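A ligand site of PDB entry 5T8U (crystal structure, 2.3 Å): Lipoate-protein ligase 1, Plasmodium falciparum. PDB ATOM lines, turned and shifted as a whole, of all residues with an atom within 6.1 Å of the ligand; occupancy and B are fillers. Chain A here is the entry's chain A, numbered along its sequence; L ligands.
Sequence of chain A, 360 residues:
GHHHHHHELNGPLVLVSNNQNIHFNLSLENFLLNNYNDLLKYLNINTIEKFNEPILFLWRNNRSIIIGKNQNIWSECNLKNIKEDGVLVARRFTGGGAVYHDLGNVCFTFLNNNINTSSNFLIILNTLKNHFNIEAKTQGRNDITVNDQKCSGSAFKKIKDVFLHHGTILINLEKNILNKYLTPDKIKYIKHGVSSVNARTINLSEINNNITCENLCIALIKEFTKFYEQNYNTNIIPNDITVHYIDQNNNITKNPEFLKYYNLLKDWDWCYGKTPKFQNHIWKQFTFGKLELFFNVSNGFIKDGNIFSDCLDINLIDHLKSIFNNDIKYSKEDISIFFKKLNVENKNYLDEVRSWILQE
An oxygen (O1) of the ligand lies within salt-bridge range of the side-chain amino group (NZ) of Lys 150, at 2.8 Å. A ring nitrogen (ND1) of His 166 lies close to a sulfur (S2) of the ligand, 3.6 Å away. The backbone NH of Gly 97 sits at hydrogen-bond distance from an oxygen (O2) of the ligand, 3.2 Å away. A ring nitrogen (NE2) of His 101 lies close to a sulfur (S2) of the ligand. S1 of the ligand lies close to NH2 of Arg 92 (3.7 Å).
NE2 of His 166 lies within hydrogen-bond range of OG1 of Thr 94 (3.0 Å). ND1 of His 166 lies close to OE2 of Glu 29 (3.4 Å). The backbone carbonyl oxygen of Gly 97 is in hydrogen-bond range of the guanidinium group of Arg 92, at 2.8 Å. N of Gly 167 sits at hydrogen-bond distance from O of Phe 108. N of Val 99 lies within hydrogen-bond range of O of Ile 66, at 2.9 Å. O of Gly 95 sits at hydrogen-bond distance from NH1 of Arg 92, at 3.2 Å. The backbone carbonyl oxygen (O) of Trp 59 lies within hydrogen-bond range of the backbone NH (N) of Cys 107, at 2.9 Å. SG of Cys 107 is in hydrogen-bond range of ND2 of Asn 61 (3.3 Å).
Merely in contact with the ligand: Ser 154 (3.0 Å), Gly 153 (3.3 Å), Gly 167 (3.4 Å), Val 99 (3.6 Å), Thr 168 (3.6 Å), Asn 142 (3.7 Å), Gly 96 (3.7 Å), Trp 59 (3.8 Å) and Cys 107 (3.96 Å). Hydrophobic or aromatic side chains within 4 Å of the ligand: Trp 59, Val 99 and His 166. 14 residues have an atom within 4 Å of the ligand: Trp 59, Arg 92, Gly 96, Gly 97, Val 99, His 101, Cys 107, Asn 142, Lys 150, Gly 153, Ser 154, His 166, Gly 167 and Thr 168. The nearest printed residue that does not touch the ligand is Ile 66 (4.1 Å).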
ATOM      1  N   ILE A  22     -16.852  -5.189  11.937  1.00  0.00           N
ATOM      2  CA  ILE A  22     -17.391  -4.204  11.008  1.00  0.00           C
ATOM      3  C   ILE A  22     -17.338  -4.716   9.575  1.00  0.00           C
ATOM      4  O   ILE A  22     -18.280  -4.535   8.803  1.00  0.00           O
ATOM      5  CB  ILE A  22     -16.635  -2.869  11.161  1.00  0.00           C
ATOM      6  CG1 ILE A  22     -17.192  -1.804  10.200  1.00  0.00           C
ATOM      7  CG2 ILE A  22     -15.132  -3.042  10.928  1.00  0.00           C
ATOM      8  CD1 ILE A  22     -18.660  -1.486  10.414  1.00  0.00           C
ATOM      9  N   LEU A  26     -20.652  -5.459   7.401  1.00  0.00           N
ATOM     10  CA  LEU A  26     -20.752  -4.728   6.132  1.00  0.00           C
ATOM     11  C   LEU A  26     -20.875  -5.684   4.962  1.00  0.00           C
ATOM     12  O   LEU A  26     -21.586  -5.381   3.988  1.00  0.00           O
ATOM     13  CB  LEU A  26     -19.544  -3.806   5.970  1.00  0.00           C
ATOM     14  CG  LEU A  26     -19.550  -2.517   6.800  1.00  0.00           C
ATOM     15  CD1 LEU A  26     -18.186  -1.845   6.745  1.00  0.00           C
ATOM     16  CD2 LEU A  26     -20.636  -1.563   6.326  1.00  0.00           C
ATOM     17  N   GLU A  29     -24.479  -6.794   4.977  1.00  0.00           N
ATOM     18  CA  GLU A  29     -25.297  -5.713   4.428  1.00  0.00           C
ATOM     19  C   GLU A  29     -25.215  -5.681   2.909  1.00  0.00           C
ATOM     20  O   GLU A  29     -26.243  -5.635   2.214  1.00  0.00           O
ATOM     21  CB  GLU A  29     -24.857  -4.378   5.026  1.00  0.00           C
ATOM     22  CG  GLU A  29     -25.687  -3.194   4.633  1.00  0.00           C
ATOM     23  CD  GLU A  29     -25.127  -1.890   5.167  1.00  0.00           C
ATOM     24  OE1 GLU A  29     -23.900  -1.701   5.089  1.00  0.00           O
ATOM     25  OE2 GLU A  29     -25.907  -1.070   5.686  1.00  0.00           O
ATOM     26  N   TRP A  59     -27.567  -4.703  13.720  1.00  0.00           N
ATOM     27  CA  TRP A  59     -26.221  -5.216  13.894  1.00  0.00           C
ATOM     28  C   TRP A  59     -25.407  -4.243  14.724  1.00  0.00           C
ATOM     29  O   TRP A  59     -25.709  -3.044  14.776  1.00  0.00           O
ATOM     30  CB  TRP A  59     -25.542  -5.466  12.540  1.00  0.00           C
ATOM     31  CG  TRP A  59     -25.738  -4.378  11.520  1.00  0.00           C
ATOM     32  CD1 TRP A  59     -26.911  -3.991  10.932  1.00  0.00           C
ATOM     33  CD2 TRP A  59     -24.718  -3.540  10.947  1.00  0.00           C
ATOM     34  NE1 TRP A  59     -26.689  -2.965  10.049  1.00  0.00           N
ATOM     35  CE2 TRP A  59     -25.356  -2.671  10.036  1.00  0.00           C
ATOM     36  CE3 TRP A  59     -23.337  -3.440  11.120  1.00  0.00           C
ATOM     37  CZ2 TRP A  59     -24.653  -1.720   9.307  1.00  0.00           C
ATOM     38  CZ3 TRP A  59     -22.643  -2.490  10.386  1.00  0.00           C
ATOM     39  CH2 TRP A  59     -23.303  -1.636   9.494  1.00  0.00           C
ATOM     40  N   ASN A  61     -21.145  -3.358  16.076  1.00  0.00           N
ATOM     41  CA  ASN A  61     -19.734  -3.517  15.739  1.00  0.00           C
ATOM     42  C   ASN A  61     -18.876  -3.065  16.906  1.00  0.00           C
ATOM     43  O   ASN A  61     -19.241  -2.153  17.652  1.00  0.00           O
ATOM     44  CB  ASN A  61     -19.351  -2.726  14.490  1.00  0.00           C
ATOM     45  CG  ASN A  61     -20.382  -2.852  13.386  1.00  0.00           C
ATOM     46  OD1 ASN A  61     -20.397  -3.819  12.627  1.00  0.00           O
ATOM     47  ND2 ASN A  61     -21.257  -1.851  13.297  1.00  0.00           N
ATOM     48  N   ILE A  66     -15.320   3.903  10.493  1.00  0.00           N
ATOM     49  CA  ILE A  66     -15.883   3.684   9.162  1.00  0.00           C
ATOM     50  C   ILE A  66     -15.871   5.032   8.454  1.00  0.00           C
ATOM     51  O   ILE A  66     -16.442   6.005   8.942  1.00  0.00           O
ATOM     52  CB  ILE A  66     -17.287   3.080   9.220  1.00  0.00           C
ATOM     53  CG1 ILE A  66     -17.288   1.799  10.060  1.00  0.00           C
ATOM     54  CG2 ILE A  66     -17.783   2.745   7.820  1.00  0.00           C
ATOM     55  CD1 ILE A  66     -17.482   2.017  11.551  1.00  0.00           C
ATOM     56  N   ARG A  92     -17.120   2.150   3.872  1.00  0.00           N
ATOM     57  CA  ARG A  92     -18.422   1.672   3.465  1.00  0.00           C
ATOM     58  C   ARG A  92     -18.710   2.076   2.020  1.00  0.00           C
ATOM     59  O   ARG A  92     -17.958   2.814   1.385  1.00  0.00           O
ATOM     60  CB  ARG A  92     -19.511   2.209   4.404  1.00  0.00           C
ATOM     61  CG  ARG A  92     -19.528   3.721   4.544  1.00  0.00           C
ATOM     62  CD  ARG A  92     -20.640   4.189   5.463  1.00  0.00           C
ATOM     63  NE  ARG A  92     -20.709   5.649   5.512  1.00  0.00           N
ATOM     64  CZ  ARG A  92     -20.018   6.416   6.347  1.00  0.00           C
ATOM     65  NH1 ARG A  92     -20.155   7.735   6.298  1.00  0.00           N
ATOM     66  NH2 ARG A  92     -19.184   5.880   7.236  1.00  0.00           N
ATOM     67  N   THR A  94     -21.571   3.657   1.090  1.00  0.00           N
ATOM     68  CA  THR A  94     -22.409   4.848   1.057  1.00  0.00           C
ATOM     69  C   THR A  94     -21.558   6.087   1.278  1.00  0.00           C
ATOM     70  O   THR A  94     -20.351   6.013   1.523  1.00  0.00           O
ATOM     71  CB  THR A  94     -23.518   4.760   2.110  1.00  0.00           C
ATOM     72  OG1 THR A  94     -22.927   4.693   3.423  1.00  0.00           O
ATOM     73  CG2 THR A  94     -24.381   3.526   1.889  1.00  0.00           C
ATOM     74  N   GLY A  95     -22.203   7.256   1.196  1.00  0.00           N
ATOM     75  CA  GLY A  95     -21.541   8.511   1.478  1.00  0.00           C
ATOM     76  C   GLY A  95     -21.605   8.862   2.955  1.00  0.00           C
ATOM     77  O   GLY A  95     -22.077   8.106   3.794  1.00  0.00           O
ATOM     78  N   GLY A  96     -21.104  10.054   3.260  1.00  0.00           N
ATOM     79  CA  GLY A  96     -21.109  10.583   4.615  1.00  0.00           C
ATOM     80  C   GLY A  96     -19.712  10.777   5.143  1.00  0.00           C
ATOM     81  O   GLY A  96     -18.706  10.623   4.426  1.00  0.00           O
ATOM     82  N   GLY A  97     -19.636  11.119   6.425  1.00  0.00           N
ATOM     83  CA  GLY A  97     -18.376  11.380   7.088  1.00  0.00           C
ATOM     84  C   GLY A  97     -17.882  10.182   7.886  1.00  0.00           C
ATOM     85  O   GLY A  97     -18.564   9.171   8.046  1.00  0.00           O
ATOM     86  N   ALA A  98     -16.661  10.328   8.401  1.00  0.00           N
ATOM     87  CA  ALA A  98     -16.058   9.270   9.197  1.00  0.00           C
ATOM     88  C   ALA A  98     -16.737   9.193  10.568  1.00  0.00           C
ATOM     89  O   ALA A  98     -16.906  10.210  11.244  1.00  0.00           O
ATOM     90  CB  ALA A  98     -14.562   9.525   9.371  1.00  0.00           C
ATOM     91  N   VAL A  99     -17.131   7.975  10.956  1.00  0.00           N
ATOM     92  CA  VAL A  99     -17.803   7.751  12.229  1.00  0.00           C
ATOM     93  C   VAL A  99     -17.090   6.642  12.982  1.00  0.00           C
ATOM     94  O   VAL A  99     -16.338   5.841  12.410  1.00  0.00           O
ATOM     95  CB  VAL A  99     -19.290   7.394  12.033  1.00  0.00           C
ATOM     96  CG1 VAL A  99     -20.042   8.566  11.413  1.00  0.00           C
ATOM     97  CG2 VAL A  99     -19.437   6.145  11.184  1.00  0.00           C
ATOM     98  N   HIS A 101     -17.501   3.419  15.876  1.00  0.00           N
ATOM     99  CA  HIS A 101     -18.442   2.404  16.341  1.00  0.00           C
ATOM    100  C   HIS A 101     -17.863   1.662  17.529  1.00  0.00           C
ATOM    101  O   HIS A 101     -16.643   1.487  17.635  1.00  0.00           O
ATOM    102  CB  HIS A 101     -18.778   1.390  15.235  1.00  0.00           C
ATOM    103  CG  HIS A 101     -19.807   1.866  14.254  1.00  0.00           C
ATOM    104  ND1 HIS A 101     -20.361   3.125  14.305  1.00  0.00           N
ATOM    105  CD2 HIS A 101     -20.381   1.243  13.200  1.00  0.00           C
ATOM    106  CE1 HIS A 101     -21.236   3.252  13.317  1.00  0.00           C
ATOM    107  NE2 HIS A 101     -21.262   2.128  12.636  1.00  0.00           N
ATOM    108  N   CYS A 107     -26.677  -0.362  14.987  1.00  0.00           N
ATOM    109  CA  CYS A 107     -26.685  -0.041  13.563  1.00  0.00           C
ATOM    110  C   CYS A 107     -27.919  -0.675  12.928  1.00  0.00           C
ATOM    111  O   CYS A 107     -28.156  -1.871  13.071  1.00  0.00           O
ATOM    112  CB  CYS A 107     -25.421  -0.553  12.866  1.00  0.00           C
ATOM    113  SG  CYS A 107     -23.879   0.211  13.418  1.00  0.00           S
ATOM    114  N   PHE A 108     -28.693   0.147  12.218  1.00  0.00           N
ATOM    115  CA  PHE A 108     -29.907  -0.289  11.553  1.00  0.00           C
ATOM    116  C   PHE A 108     -29.741  -0.140  10.040  1.00  0.00           C
ATOM    117  O   PHE A 108     -29.057   0.768   9.556  1.00  0.00           O
ATOM    118  CB  PHE A 108     -31.127   0.529  12.025  1.00  0.00           C
ATOM    119  CG  PHE A 108     -31.044   1.992  11.673  1.00  0.00           C
ATOM    120  CD1 PHE A 108     -31.567   2.459  10.476  1.00  0.00           C
ATOM    121  CD2 PHE A 108     -30.468   2.903  12.552  1.00  0.00           C
ATOM    122  CE1 PHE A 108     -31.504   3.808  10.151  1.00  0.00           C
ATOM    123  CE2 PHE A 108     -30.408   4.245  12.233  1.00  0.00           C
ATOM    124  CZ  PHE A 108     -30.922   4.697  11.027  1.00  0.00           C
ATOM    125  N   ASN A 142     -30.433  13.102   7.158  1.00  0.00           N
ATOM    126  CA  ASN A 142     -29.700  11.933   7.639  1.00  0.00           C
ATOM    127  C   ASN A 142     -29.437  11.927   9.140  1.00  0.00           C
ATOM    128  O   ASN A 142     -28.681  11.067   9.611  1.00  0.00           O
ATOM    129  CB  ASN A 142     -28.359  11.834   6.912  1.00  0.00           C
ATOM    130  CG  ASN A 142     -27.383  12.917   7.335  1.00  0.00           C
ATOM    131  OD1 ASN A 142     -27.732  14.095   7.373  1.00  0.00           O
ATOM    132  ND2 ASN A 142     -26.156  12.511   7.662  1.00  0.00           N
ATOM    133  N   ASP A 143     -30.007  12.850   9.919  1.00  0.00           N
ATOM    134  CA  ASP A 143     -29.681  12.961  11.329  1.00  0.00           C
ATOM    135  C   ASP A 143     -30.937  12.998  12.183  1.00  0.00           C
ATOM    136  O   ASP A 143     -31.999  13.473  11.750  1.00  0.00           O
ATOM    137  CB  ASP A 143     -28.847  14.220  11.605  1.00  0.00           C
ATOM    138  CG  ASP A 143     -27.399  14.067  11.173  1.00  0.00           C
ATOM    139  OD1 ASP A 143     -27.093  13.045  10.512  1.00  0.00           O
ATOM    140  OD2 ASP A 143     -26.583  14.942  11.492  1.00  0.00           O
ATOM    141  N   LYS A 150     -26.915  15.382  18.133  1.00  0.00           N
ATOM    142  CA  LYS A 150     -26.979  14.180  17.311  1.00  0.00           C
ATOM    143  C   LYS A 150     -27.044  12.933  18.183  1.00  0.00           C
ATOM    144  O   LYS A 150     -26.228  12.755  19.092  1.00  0.00           O
ATOM    145  CB  LYS A 150     -25.754  14.102  16.387  1.00  0.00           C
ATOM    146  CG  LYS A 150     -25.933  13.174  15.203  1.00  0.00           C
ATOM    147  CD  LYS A 150     -24.618  12.534  14.759  1.00  0.00           C
ATOM    148  CE  LYS A 150     -24.330  12.787  13.289  1.00  0.00           C
ATOM    149  NZ  LYS A 150     -23.267  11.889  12.767  1.00  0.00           N
ATOM    150  N   SER A 152     -28.272   9.971  16.178  1.00  0.00           N
ATOM    151  CA  SER A 152     -28.267   8.977  15.119  1.00  0.00           C
ATOM    152  C   SER A 152     -27.777   9.624  13.839  1.00  0.00           C
ATOM    153  O   SER A 152     -27.961  10.825  13.620  1.00  0.00           O
ATOM    154  CB  SER A 152     -29.664   8.370  14.910  1.00  0.00           C
ATOM    155  OG  SER A 152     -29.796   7.832  13.601  1.00  0.00           O
ATOM    156  N   GLY A 153     -27.134   8.822  12.991  1.00  0.00           N
ATOM    157  CA  GLY A 153     -26.587   9.322  11.739  1.00  0.00           C
ATOM    158  C   GLY A 153     -26.714   8.341  10.601  1.00  0.00           C
ATOM    159  O   GLY A 153     -26.235   7.200  10.706  1.00  0.00           O
ATOM    160  N   SER A 154     -27.338   8.744   9.502  1.00  0.00           N
ATOM    161  CA  SER A 154     -27.723   7.832   8.444  1.00  0.00           C
ATOM    162  C   SER A 154     -26.961   8.098   7.152  1.00  0.00           C
ATOM    163  O   SER A 154     -26.346   9.148   6.953  1.00  0.00           O
ATOM    164  CB  SER A 154     -29.234   7.936   8.173  1.00  0.00           C
ATOM    165  OG  SER A 154     -29.971   7.629   9.348  1.00  0.00           O
ATOM    166  N   ALA A 155     -27.011   7.098   6.270  1.00  0.00           N
ATOM    167  CA  ALA A 155     -26.439   7.196   4.928  1.00  0.00           C
ATOM    168  C   ALA A 155     -27.232   6.266   4.016  1.00  0.00           C
ATOM    169  O   ALA A 155     -27.897   5.329   4.480  1.00  0.00           O
ATOM    170  CB  ALA A 155     -24.949   6.854   4.908  1.00  0.00           C
ATOM    171  N   HIS A 166     -29.097   2.974   5.751  1.00  0.00           N
ATOM    172  CA  HIS A 166     -28.485   2.393   6.936  1.00  0.00           C
ATOM    173  C   HIS A 166     -27.853   3.497   7.767  1.00  0.00           C
ATOM    174  O   HIS A 166     -27.128   4.353   7.235  1.00  0.00           O
ATOM    175  CB  HIS A 166     -27.438   1.332   6.557  1.00  0.00           C
ATOM    176  CG  HIS A 166     -26.103   1.881   6.158  1.00  0.00           C
ATOM    177  ND1 HIS A 166     -25.049   1.974   7.033  1.00  0.00           N
ATOM    178  CD2 HIS A 166     -25.652   2.342   4.972  1.00  0.00           C
ATOM    179  CE1 HIS A 166     -23.998   2.481   6.413  1.00  0.00           C
ATOM    180  NE2 HIS A 166     -24.339   2.708   5.155  1.00  0.00           N
ATOM    181  N   GLY A 167     -28.133   3.475   9.069  1.00  0.00           N
ATOM    182  CA  GLY A 167     -27.672   4.514   9.976  1.00  0.00           C
ATOM    183  C   GLY A 167     -27.320   3.934  11.336  1.00  0.00           C
ATOM    184  O   GLY A 167     -27.479   2.730  11.582  1.00  0.00           O
ATOM    185  N   THR A 168     -26.844   4.813  12.210  1.00  0.00           N
ATOM    186  CA  THR A 168     -26.391   4.441  13.542  1.00  0.00           C
ATOM    187  C   THR A 168     -27.261   5.128  14.585  1.00  0.00           C
ATOM    188  O   THR A 168     -27.653   6.285  14.418  1.00  0.00           O
ATOM    189  CB  THR A 168     -24.927   4.834  13.764  1.00  0.00           C
ATOM    190  OG1 THR A 168     -24.509   4.434  15.066  1.00  0.00           O
ATOM    191  CG2 THR A 168     -24.738   6.339  13.608  1.00  0.00           C
ATOM    192  N   ASP A 310     -17.522  14.710   1.329  1.00  0.00           N
ATOM    193  CA  ASP A 310     -18.242  14.413   2.566  1.00  0.00           C
ATOM    194  C   ASP A 310     -19.738  14.205   2.304  1.00  0.00           C
ATOM    195  O   ASP A 310     -20.539  14.242   3.240  1.00  0.00           O
ATOM    196  CB  ASP A 310     -18.025  15.551   3.560  1.00  0.00           C
ATOM    197  CG  ASP A 310     -18.223  15.117   4.998  1.00  0.00           C
ATOM    198  OD1 ASP A 310     -17.740  14.039   5.375  1.00  0.00           O
ATOM    199  OD2 ASP A 310     -18.845  15.890   5.768  1.00  0.00           O
ATOM    200  N   LEU A 312     -23.578  12.923   0.863  1.00  0.00           N
ATOM    201  CA  LEU A 312     -24.469  11.766   0.884  1.00  0.00           C
ATOM    202  C   LEU A 312     -24.876  11.319  -0.511  1.00  0.00           C
ATOM    203  O   LEU A 312     -25.213  10.137  -0.699  1.00  0.00           O
ATOM    204  CB  LEU A 312     -25.730  12.083   1.686  1.00  0.00           C
ATOM    205  CG  LEU A 312     -25.582  12.288   3.193  1.00  0.00           C
ATOM    206  CD1 LEU A 312     -26.891  12.795   3.776  1.00  0.00           C
ATOM    207  CD2 LEU A 312     -25.156  10.998   3.883  1.00  0.00           C
HETATM  208  C1  LIG L   1     -23.159  10.784   8.868  1.00  0.00           C
HETATM  209  O1  LIG L   1     -23.287  11.316  10.004  1.00  0.00           O
HETATM  210  C2  LIG L   1     -23.813   9.443   8.580  1.00  0.00           C
HETATM  211  O2  LIG L   1     -22.484  11.368   7.969  1.00  0.00           O
HETATM  212  C3  LIG L   1     -23.116   8.353   9.389  1.00  0.00           C
HETATM  213  C4  LIG L   1     -23.492   6.974   8.853  1.00  0.00           C
HETATM  214  C5  LIG L   1     -22.557   5.936   9.470  1.00  0.00           C
HETATM  215  C6  LIG L   1     -22.792   4.662   8.911  1.00  0.00           C
HETATM  216  S1  LIG L   1     -21.543   3.778   9.116  1.00  0.00           S
HETATM  217  C7  LIG L   1     -24.277   3.764   9.858  1.00  0.00           C
HETATM  218  C8  LIG L   1     -23.920   2.214  10.006  1.00  0.00           C
HETATM  219  S2  LIG L   1     -22.230   1.998   9.314  1.00  0.00           S
